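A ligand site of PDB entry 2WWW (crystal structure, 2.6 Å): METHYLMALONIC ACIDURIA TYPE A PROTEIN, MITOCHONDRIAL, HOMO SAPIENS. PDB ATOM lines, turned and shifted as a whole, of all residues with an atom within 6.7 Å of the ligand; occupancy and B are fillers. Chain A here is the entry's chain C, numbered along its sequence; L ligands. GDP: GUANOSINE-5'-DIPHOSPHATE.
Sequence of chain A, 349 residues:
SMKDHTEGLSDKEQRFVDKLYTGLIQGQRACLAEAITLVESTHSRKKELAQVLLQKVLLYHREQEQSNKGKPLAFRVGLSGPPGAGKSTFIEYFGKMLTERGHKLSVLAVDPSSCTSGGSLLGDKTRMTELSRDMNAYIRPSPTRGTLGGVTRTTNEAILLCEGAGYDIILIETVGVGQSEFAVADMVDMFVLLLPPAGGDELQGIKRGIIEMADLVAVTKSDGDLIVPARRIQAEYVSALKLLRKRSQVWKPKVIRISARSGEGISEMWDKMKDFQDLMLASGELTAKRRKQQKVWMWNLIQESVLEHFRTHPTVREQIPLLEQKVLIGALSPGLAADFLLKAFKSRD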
ATOM      1  N   GLY A  81      -5.485  -1.351  -4.599  1.00  0.00           N
ATOM      2  CA  GLY A  81      -4.986  -2.086  -3.440  1.00  0.00           C
ATOM      3  C   GLY A  81      -3.514  -1.842  -3.209  1.00  0.00           C
ATOM      4  O   GLY A  81      -2.840  -1.289  -4.064  1.00  0.00           O
ATOM      5  N   PRO A  82      -2.989  -2.272  -2.061  1.00  0.00           N
ATOM      6  CA  PRO A  82      -1.530  -2.120  -1.809  1.00  0.00           C
ATOM      7  C   PRO A  82      -0.667  -3.007  -2.756  1.00  0.00           C
ATOM      8  O   PRO A  82      -1.216  -3.940  -3.370  1.00  0.00           O
ATOM      9  CB  PRO A  82      -1.372  -2.595  -0.362  1.00  0.00           C
ATOM     10  CG  PRO A  82      -2.749  -2.811   0.191  1.00  0.00           C
ATOM     11  CD  PRO A  82      -3.659  -2.978  -0.942  1.00  0.00           C
ATOM     12  N   PRO A  83       0.657  -2.774  -2.871  1.00  0.00           N
ATOM     13  CA  PRO A  83       1.489  -3.691  -3.693  1.00  0.00           C
ATOM     14  C   PRO A  83       1.507  -5.076  -3.014  1.00  0.00           C
ATOM     15  O   PRO A  83       1.548  -5.149  -1.769  1.00  0.00           O
ATOM     16  CB  PRO A  83       2.887  -3.047  -3.635  1.00  0.00           C
ATOM     17  CG  PRO A  83       2.641  -1.629  -3.167  1.00  0.00           C
ATOM     18  CD  PRO A  83       1.493  -1.725  -2.239  1.00  0.00           C
ATOM     19  N   GLY A  84       1.422  -6.153  -3.785  1.00  0.00           N
ATOM     20  CA  GLY A  84       1.358  -7.501  -3.231  1.00  0.00           C
ATOM     21  C   GLY A  84      -0.046  -7.994  -2.817  1.00  0.00           C
ATOM     22  O   GLY A  84      -0.177  -9.148  -2.368  1.00  0.00           O
ATOM     23  N   ALA A  85      -1.130  -7.143  -2.965  1.00  0.00           N
ATOM     24  CA  ALA A  85      -2.514  -7.488  -2.614  1.00  0.00           C
ATOM     25  C   ALA A  85      -2.990  -8.672  -3.435  1.00  0.00           C
ATOM     26  O   ALA A  85      -3.763  -9.460  -2.921  1.00  0.00           O
ATOM     27  CB  ALA A  85      -3.450  -6.314  -2.802  1.00  0.00           C
ATOM     28  N   GLY A  86      -2.516  -8.831  -4.666  1.00  0.00           N
ATOM     29  CA  GLY A  86      -2.912  -9.951  -5.508  1.00  0.00           C
ATOM     30  C   GLY A  86      -3.650  -9.485  -6.728  1.00  0.00           C
ATOM     31  O   GLY A  86      -4.387 -10.272  -7.354  1.00  0.00           O
ATOM     32  N   LYS A  87      -3.467  -8.159  -7.059  1.00  0.00           N
ATOM     33  CA  LYS A  87      -4.106  -7.454  -8.167  1.00  0.00           C
ATOM     34  C   LYS A  87      -3.859  -8.077  -9.536  1.00  0.00           C
ATOM     35  O   LYS A  87      -4.811  -8.516 -10.198  1.00  0.00           O
ATOM     36  CB  LYS A  87      -3.761  -5.957  -8.177  1.00  0.00           C
ATOM     37  CG  LYS A  87      -4.220  -5.134  -6.941  1.00  0.00           C
ATOM     38  CD  LYS A  87      -3.986  -3.608  -7.197  1.00  0.00           C
ATOM     39  CE  LYS A  87      -2.636  -3.029  -6.733  1.00  0.00           C
ATOM     40  NZ  LYS A  87      -1.424  -3.817  -7.127  1.00  0.00           N
ATOM     41  N   SER A  88      -2.610  -8.157  -9.926  1.00  0.00           N
ATOM     42  CA  SER A  88      -2.167  -8.752 -11.195  1.00  0.00           C
ATOM     43  C   SER A  88      -2.689 -10.177 -11.373  1.00  0.00           C
ATOM     44  O   SER A  88      -3.214 -10.535 -12.423  1.00  0.00           O
ATOM     45  CB  SER A  88      -0.640  -8.770 -11.258  1.00  0.00           C
ATOM     46  OG  SER A  88      -0.040  -7.539 -10.853  1.00  0.00           O
ATOM     47  N   THR A  89      -2.557 -10.998 -10.321  1.00  0.00           N
ATOM     48  CA  THR A  89      -2.985 -12.411 -10.304  1.00  0.00           C
ATOM     49  C   THR A  89      -4.548 -12.460 -10.406  1.00  0.00           C
ATOM     50  O   THR A  89      -5.076 -13.388 -11.029  1.00  0.00           O
ATOM     51  CB  THR A  89      -2.441 -13.101  -9.012  1.00  0.00           C
ATOM     52  OG1 THR A  89      -1.037 -12.899  -8.886  1.00  0.00           O
ATOM     53  CG2 THR A  89      -2.720 -14.577  -8.945  1.00  0.00           C
ATOM     54  N   PHE A  90      -5.255 -11.453  -9.801  1.00  0.00           N
ATOM     55  CA  PHE A  90      -6.692 -11.344  -9.811  1.00  0.00           C
ATOM     56  C   PHE A  90      -7.184 -10.982 -11.198  1.00  0.00           C
ATOM     57  O   PHE A  90      -8.119 -11.626 -11.674  1.00  0.00           O
ATOM     58  CB  PHE A  90      -7.192 -10.290  -8.787  1.00  0.00           C
ATOM     59  CG  PHE A  90      -8.653  -9.911  -8.966  1.00  0.00           C
ATOM     60  CD1 PHE A  90      -9.661 -10.762  -8.534  1.00  0.00           C
ATOM     61  CD2 PHE A  90      -9.003  -8.740  -9.624  1.00  0.00           C
ATOM     62  CE1 PHE A  90     -11.005 -10.448  -8.766  1.00  0.00           C
ATOM     63  CE2 PHE A  90     -10.342  -8.434  -9.852  1.00  0.00           C
ATOM     64  CZ  PHE A  90     -11.327  -9.288  -9.426  1.00  0.00           C
ATOM     65  N   GLU A 173      -6.697  -0.087 -13.268  1.00  0.00           N
ATOM     66  CA  GLU A 173      -5.895  -0.618 -12.174  1.00  0.00           C
ATOM     67  C   GLU A 173      -4.944   0.469 -11.601  1.00  0.00           C
ATOM     68  O   GLU A 173      -4.293   1.166 -12.352  1.00  0.00           O
ATOM     69  CB  GLU A 173      -5.137  -1.854 -12.653  1.00  0.00           C
ATOM     70  CG  GLU A 173      -4.370  -2.549 -11.548  1.00  0.00           C
ATOM     71  CD  GLU A 173      -3.188  -3.393 -12.012  1.00  0.00           C
ATOM     72  OE1 GLU A 173      -2.854  -3.344 -13.215  1.00  0.00           O
ATOM     73  OE2 GLU A 173      -2.608  -4.110 -11.158  1.00  0.00           O
ATOM     74  N   VAL A 175      -2.609   1.632  -7.551  1.00  0.00           N
ATOM     75  CA  VAL A 175      -1.941   1.223  -6.289  1.00  0.00           C
ATOM     76  C   VAL A 175      -2.244   2.233  -5.193  1.00  0.00           C
ATOM     77  O   VAL A 175      -2.265   3.453  -5.444  1.00  0.00           O
ATOM     78  CB  VAL A 175      -0.396   1.001  -6.402  1.00  0.00           C
ATOM     79  CG1 VAL A 175       0.109   0.038  -5.308  1.00  0.00           C
ATOM     80  CG2 VAL A 175       0.012   0.507  -7.779  1.00  0.00           C
ATOM     81  N   THR A 220      -8.260 -10.639  -0.305  1.00  0.00           N
ATOM     82  CA  THR A 220      -7.512 -11.541  -1.169  1.00  0.00           C
ATOM     83  C   THR A 220      -6.806 -12.651  -0.418  1.00  0.00           C
ATOM     84  O   THR A 220      -6.768 -12.646   0.819  1.00  0.00           O
ATOM     85  CB  THR A 220      -6.569 -10.738  -2.059  1.00  0.00           C
ATOM     86  OG1 THR A 220      -5.765  -9.980  -1.196  1.00  0.00           O
ATOM     87  CG2 THR A 220      -7.289  -9.764  -2.990  1.00  0.00           C
ATOM     88  N   LYS A 221      -6.283 -13.638  -1.214  1.00  0.00           N
ATOM     89  CA  LYS A 221      -5.487 -14.797  -0.796  1.00  0.00           C
ATOM     90  C   LYS A 221      -6.181 -15.641   0.251  1.00  0.00           C
ATOM     91  O   LYS A 221      -5.516 -16.303   1.034  1.00  0.00           O
ATOM     92  CB  LYS A 221      -4.100 -14.346  -0.311  1.00  0.00           C
ATOM     93  CG  LYS A 221      -3.392 -13.365  -1.254  1.00  0.00           C
ATOM     94  CD  LYS A 221      -2.141 -12.811  -0.637  1.00  0.00           C
ATOM     95  CE  LYS A 221      -1.410 -11.929  -1.615  1.00  0.00           C
ATOM     96  NZ  LYS A 221       0.011 -11.670  -1.193  1.00  0.00           N
ATOM     97  N   SER A 222      -7.523 -15.668   0.264  1.00  0.00           N
ATOM     98  CA  SER A 222      -8.339 -16.437   1.208  1.00  0.00           C
ATOM     99  C   SER A 222      -8.236 -17.950   0.912  1.00  0.00           C
ATOM    100  O   SER A 222      -9.251 -18.614   0.657  1.00  0.00           O
ATOM    101  CB  SER A 222      -9.781 -15.911   1.204  1.00  0.00           C
ATOM    102  OG  SER A 222     -10.574 -16.587   2.171  1.00  0.00           O
ATOM    103  N   ASP A 223      -6.987 -18.489   0.951  1.00  0.00           N
ATOM    104  CA  ASP A 223      -6.627 -19.890   0.670  1.00  0.00           C
ATOM    105  C   ASP A 223      -5.635 -20.428   1.658  1.00  0.00           C
ATOM    106  O   ASP A 223      -4.841 -19.644   2.219  1.00  0.00           O
ATOM    107  CB  ASP A 223      -6.064 -20.051  -0.761  1.00  0.00           C
ATOM    108  CG  ASP A 223      -5.019 -19.017  -1.190  1.00  0.00           C
ATOM    109  OD1 ASP A 223      -5.247 -18.324  -2.190  1.00  0.00           O
ATOM    110  OD2 ASP A 223      -3.997 -18.898  -0.516  1.00  0.00           O
ATOM    111  N   GLY A 224      -5.662 -21.759   1.845  1.00  0.00           N
ATOM    112  CA  GLY A 224      -4.737 -22.482   2.729  1.00  0.00           C
ATOM    113  C   GLY A 224      -4.668 -21.950   4.154  1.00  0.00           C
ATOM    114  O   GLY A 224      -5.705 -21.854   4.813  1.00  0.00           O
ATOM    115  N   LEU A 226      -4.225 -18.924   5.139  1.00  0.00           N
ATOM    116  CA  LEU A 226      -4.584 -17.498   5.185  1.00  0.00           C
ATOM    117  C   LEU A 226      -6.080 -17.334   5.199  1.00  0.00           C
ATOM    118  O   LEU A 226      -6.558 -16.199   5.169  1.00  0.00           O
ATOM    119  CB  LEU A 226      -3.934 -16.677   4.053  1.00  0.00           C
ATOM    120  CG  LEU A 226      -2.433 -16.351   4.172  1.00  0.00           C
ATOM    121  CD1 LEU A 226      -1.922 -15.682   2.921  1.00  0.00           C
ATOM    122  CD2 LEU A 226      -2.124 -15.453   5.373  1.00  0.00           C
ATOM    123  N   ILE A 258     -11.786 -13.615  -1.446  1.00  0.00           N
ATOM    124  CA  ILE A 258     -11.521 -14.251  -2.731  1.00  0.00           C
ATOM    125  C   ILE A 258     -10.157 -14.944  -2.701  1.00  0.00           C
ATOM    126  O   ILE A 258      -9.365 -14.687  -1.804  1.00  0.00           O
ATOM    127  CB  ILE A 258     -11.616 -13.223  -3.940  1.00  0.00           C
ATOM    128  CG1 ILE A 258     -10.446 -12.202  -3.921  1.00  0.00           C
ATOM    129  CG2 ILE A 258     -13.024 -12.555  -4.034  1.00  0.00           C
ATOM    130  CD1 ILE A 258     -10.469 -11.209  -4.964  1.00  0.00           C
ATOM    131  N   SER A 259      -9.906 -15.793  -3.704  1.00  0.00           N
ATOM    132  CA  SER A 259      -8.612 -16.426  -3.946  1.00  0.00           C
ATOM    133  C   SER A 259      -8.528 -16.719  -5.444  1.00  0.00           C
ATOM    134  O   SER A 259      -9.376 -17.431  -5.976  1.00  0.00           O
ATOM    135  CB  SER A 259      -8.439 -17.671  -3.086  1.00  0.00           C
ATOM    136  OG  SER A 259      -7.412 -18.536  -3.569  1.00  0.00           O
ATOM    137  N   ALA A 260      -7.577 -16.076  -6.144  1.00  0.00           N
ATOM    138  CA  ALA A 260      -7.292 -16.302  -7.567  1.00  0.00           C
ATOM    139  C   ALA A 260      -6.595 -17.648  -7.702  1.00  0.00           C
ATOM    140  O   ALA A 260      -6.614 -18.270  -8.771  1.00  0.00           O
ATOM    141  CB  ALA A 260      -6.398 -15.203  -8.121  1.00  0.00           C
ATOM    142  N   ARG A 261      -5.984 -18.123  -6.608  1.00  0.00           N
ATOM    143  CA  ARG A 261      -5.277 -19.398  -6.541  1.00  0.00           C
ATOM    144  C   ARG A 261      -6.285 -20.532  -6.501  1.00  0.00           C
ATOM    145  O   ARG A 261      -6.159 -21.470  -7.287  1.00  0.00           O
ATOM    146  CB  ARG A 261      -4.388 -19.400  -5.315  1.00  0.00           C
ATOM    147  CG  ARG A 261      -3.237 -20.347  -5.368  1.00  0.00           C
ATOM    148  CD  ARG A 261      -2.052 -19.841  -4.582  1.00  0.00           C
ATOM    149  NE  ARG A 261      -1.283 -18.853  -5.334  1.00  0.00           N
ATOM    150  CZ  ARG A 261      -0.073 -18.446  -5.004  1.00  0.00           C
ATOM    151  NH1 ARG A 261       0.517 -17.499  -5.718  1.00  0.00           N
ATOM    152  NH2 ARG A 261       0.548 -18.943  -3.944  1.00  0.00           N
ATOM    153  N   SER A 262      -7.337 -20.429  -5.653  1.00  0.00           N
ATOM    154  CA  SER A 262      -8.367 -21.468  -5.565  1.00  0.00           C
ATOM    155  C   SER A 262      -9.604 -21.166  -6.379  1.00  0.00           C
ATOM    156  O   SER A 262     -10.378 -22.066  -6.612  1.00  0.00           O
ATOM    157  CB  SER A 262      -8.738 -21.749  -4.099  1.00  0.00           C
ATOM    158  OG  SER A 262      -9.441 -20.705  -3.442  1.00  0.00           O
ATOM    159  N   GLY A 263      -9.819 -19.907  -6.744  1.00  0.00           N
ATOM    160  CA  GLY A 263     -11.004 -19.455  -7.464  1.00  0.00           C
ATOM    161  C   GLY A 263     -12.140 -19.027  -6.546  1.00  0.00           C
ATOM    162  O   GLY A 263     -13.158 -18.461  -6.998  1.00  0.00           O
HETATM  163  PB  GDP L   1       0.220  -7.034  -6.942  1.00  0.00           P
HETATM  164  O1B GDP L   1      -0.123  -6.924  -8.405  1.00  0.00           O
HETATM  165  O2B GDP L   1      -0.874  -6.361  -6.183  1.00  0.00           O
HETATM  166  O3B GDP L   1       1.507  -6.316  -6.606  1.00  0.00           O
HETATM  167  O3A GDP L   1       0.270  -8.582  -6.445  1.00  0.00           O
HETATM  168  PA  GDP L   1       0.520  -9.907  -7.369  1.00  0.00           P
HETATM  169  O1A GDP L   1      -0.691 -10.331  -8.158  1.00  0.00           O
HETATM  170  O2A GDP L   1       1.656  -9.786  -8.307  1.00  0.00           O
HETATM  171  O5' GDP L   1       0.805 -11.014  -6.238  1.00  0.00           O
HETATM  172  C5' GDP L   1       1.464 -10.709  -4.993  1.00  0.00           C
HETATM  173  C4' GDP L   1       1.988 -11.997  -4.348  1.00  0.00           C
HETATM  174  O4' GDP L   1       0.895 -12.711  -3.766  1.00  0.00           O
HETATM  175  C3' GDP L   1       2.619 -12.929  -5.395  1.00  0.00           C
HETATM  176  O3' GDP L   1       3.738 -13.668  -4.849  1.00  0.00           O
HETATM  177  C2' GDP L   1       1.463 -13.859  -5.726  1.00  0.00           C
HETATM  178  O2' GDP L   1       1.884 -15.129  -6.230  1.00  0.00           O
HETATM  179  C1' GDP L   1       0.693 -13.965  -4.416  1.00  0.00           C
HETATM  180  N9  GDP L   1      -0.750 -14.225  -4.658  1.00  0.00           N
HETATM  181  C8  GDP L   1      -1.533 -13.594  -5.547  1.00  0.00           C
HETATM  182  N7  GDP L   1      -2.799 -14.096  -5.506  1.00  0.00           N
HETATM  183  C5  GDP L   1      -2.837 -15.074  -4.576  1.00  0.00           C
HETATM  184  C6  GDP L   1      -3.860 -15.964  -3.981  1.00  0.00           C
HETATM  185  O6  GDP L   1      -5.050 -15.959  -4.395  1.00  0.00           O
HETATM  186  N1  GDP L   1      -3.438 -16.842  -3.062  1.00  0.00           N
HETATM  187  C2  GDP L   1      -2.178 -16.832  -2.555  1.00  0.00           C
HETATM  188  N2  GDP L   1      -1.825 -17.680  -1.552  1.00  0.00           N
HETATM  189  N3  GDP L   1      -1.222 -16.012  -3.028  1.00  0.00           N
HETATM  190  C4  GDP L   1      -1.470 -15.155  -4.038  1.00  0.00           C
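N of Arg 261 sits close to OG of Ser 259.
N of Ser 262 lies within hydrogen-bond range of OG of Ser 259 (2.8 Å).
O of Ile 258 is in hydrogen-bond range of N of Lys 221 (3.3 Å).
O of Gly 84 sits at hydrogen-bond distance from NZ of Lys 221.
The backbone carbonyl oxygen (O) of Ala 85 sits at hydrogen-bond distance from the side-chain hydroxyl (OG1) of Thr 220.
The side-chain hydroxyl (OG) of Ser 259 is in hydrogen-bond range of the side-chain carboxylate (OD1) of Asp 223.
Merely in contact with the ligand: Pro 82, Pro 83 and Ser 259.
13 residues have an atom within 4 Å of the ligand: Pro 82, Pro 83, Gly 84, Ala 85, Gly 86, Lys 87, Ser 88, Thr 89, Lys 221, Asp 223, Ser 259, Ala 260 and Arg 261.
The nearest printed residue that does not touch the ligand is Glu 173 (4.7 Å).
The guanidinium group (NH1) of Arg 261 lies within hydrogen-bond range of an oxygen (O2') of the ligand (2.8 Å).
N of Ala 260 sits at hydrogen-bond distance from O6 of the ligand (3.1 Å).
An oxygen (O2B) of the ligand lies within salt-bridge range of the side-chain amino group (NZ) of Lys 87 (2.8 Å).
An oxygen (O3A) of the ligand lies within hydrogen-bond range of the backbone NH of Gly 86 (3.3 Å).
O6 of the ligand sits at hydrogen-bond distance from N of Arg 261 (3.2 Å).
The side-chain carboxylate (OD1) of Asp 223 is in hydrogen-bond range of a nitrogen (N1) of the ligand (2.5 Å).
O4' of the ligand sits at hydrogen-bond distance from NZ of Lys 221, at 2.9 Å.
The backbone NH (N) of Ser 88 lies within hydrogen-bond range of an oxygen (O1B) of the ligand (3.2 Å).
An oxygen (O2B) of the ligand lies within hydrogen-bond range of the backbone NH (N) of Lys 87.
The side-chain hydroxyl (OG1) of Thr 89 is in hydrogen-bond range of an oxygen (O1A) of the ligand (2.7 Å).
The backbone NH (N) of Thr 89 is in hydrogen-bond range of an oxygen (O1A) of the ligand, 2.9 Å away.
OG of Ser 88 lies within hydrogen-bond range of O1B of the ligand, 2.5 Å away.
An oxygen (O3B) of the ligand is in hydrogen-bond range of the backbone NH (N) of Gly 84, at 2.8 Å.
The backbone NH (N) of Ala 85 sits at hydrogen-bond distance from an oxygen (O2B) of the ligand.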
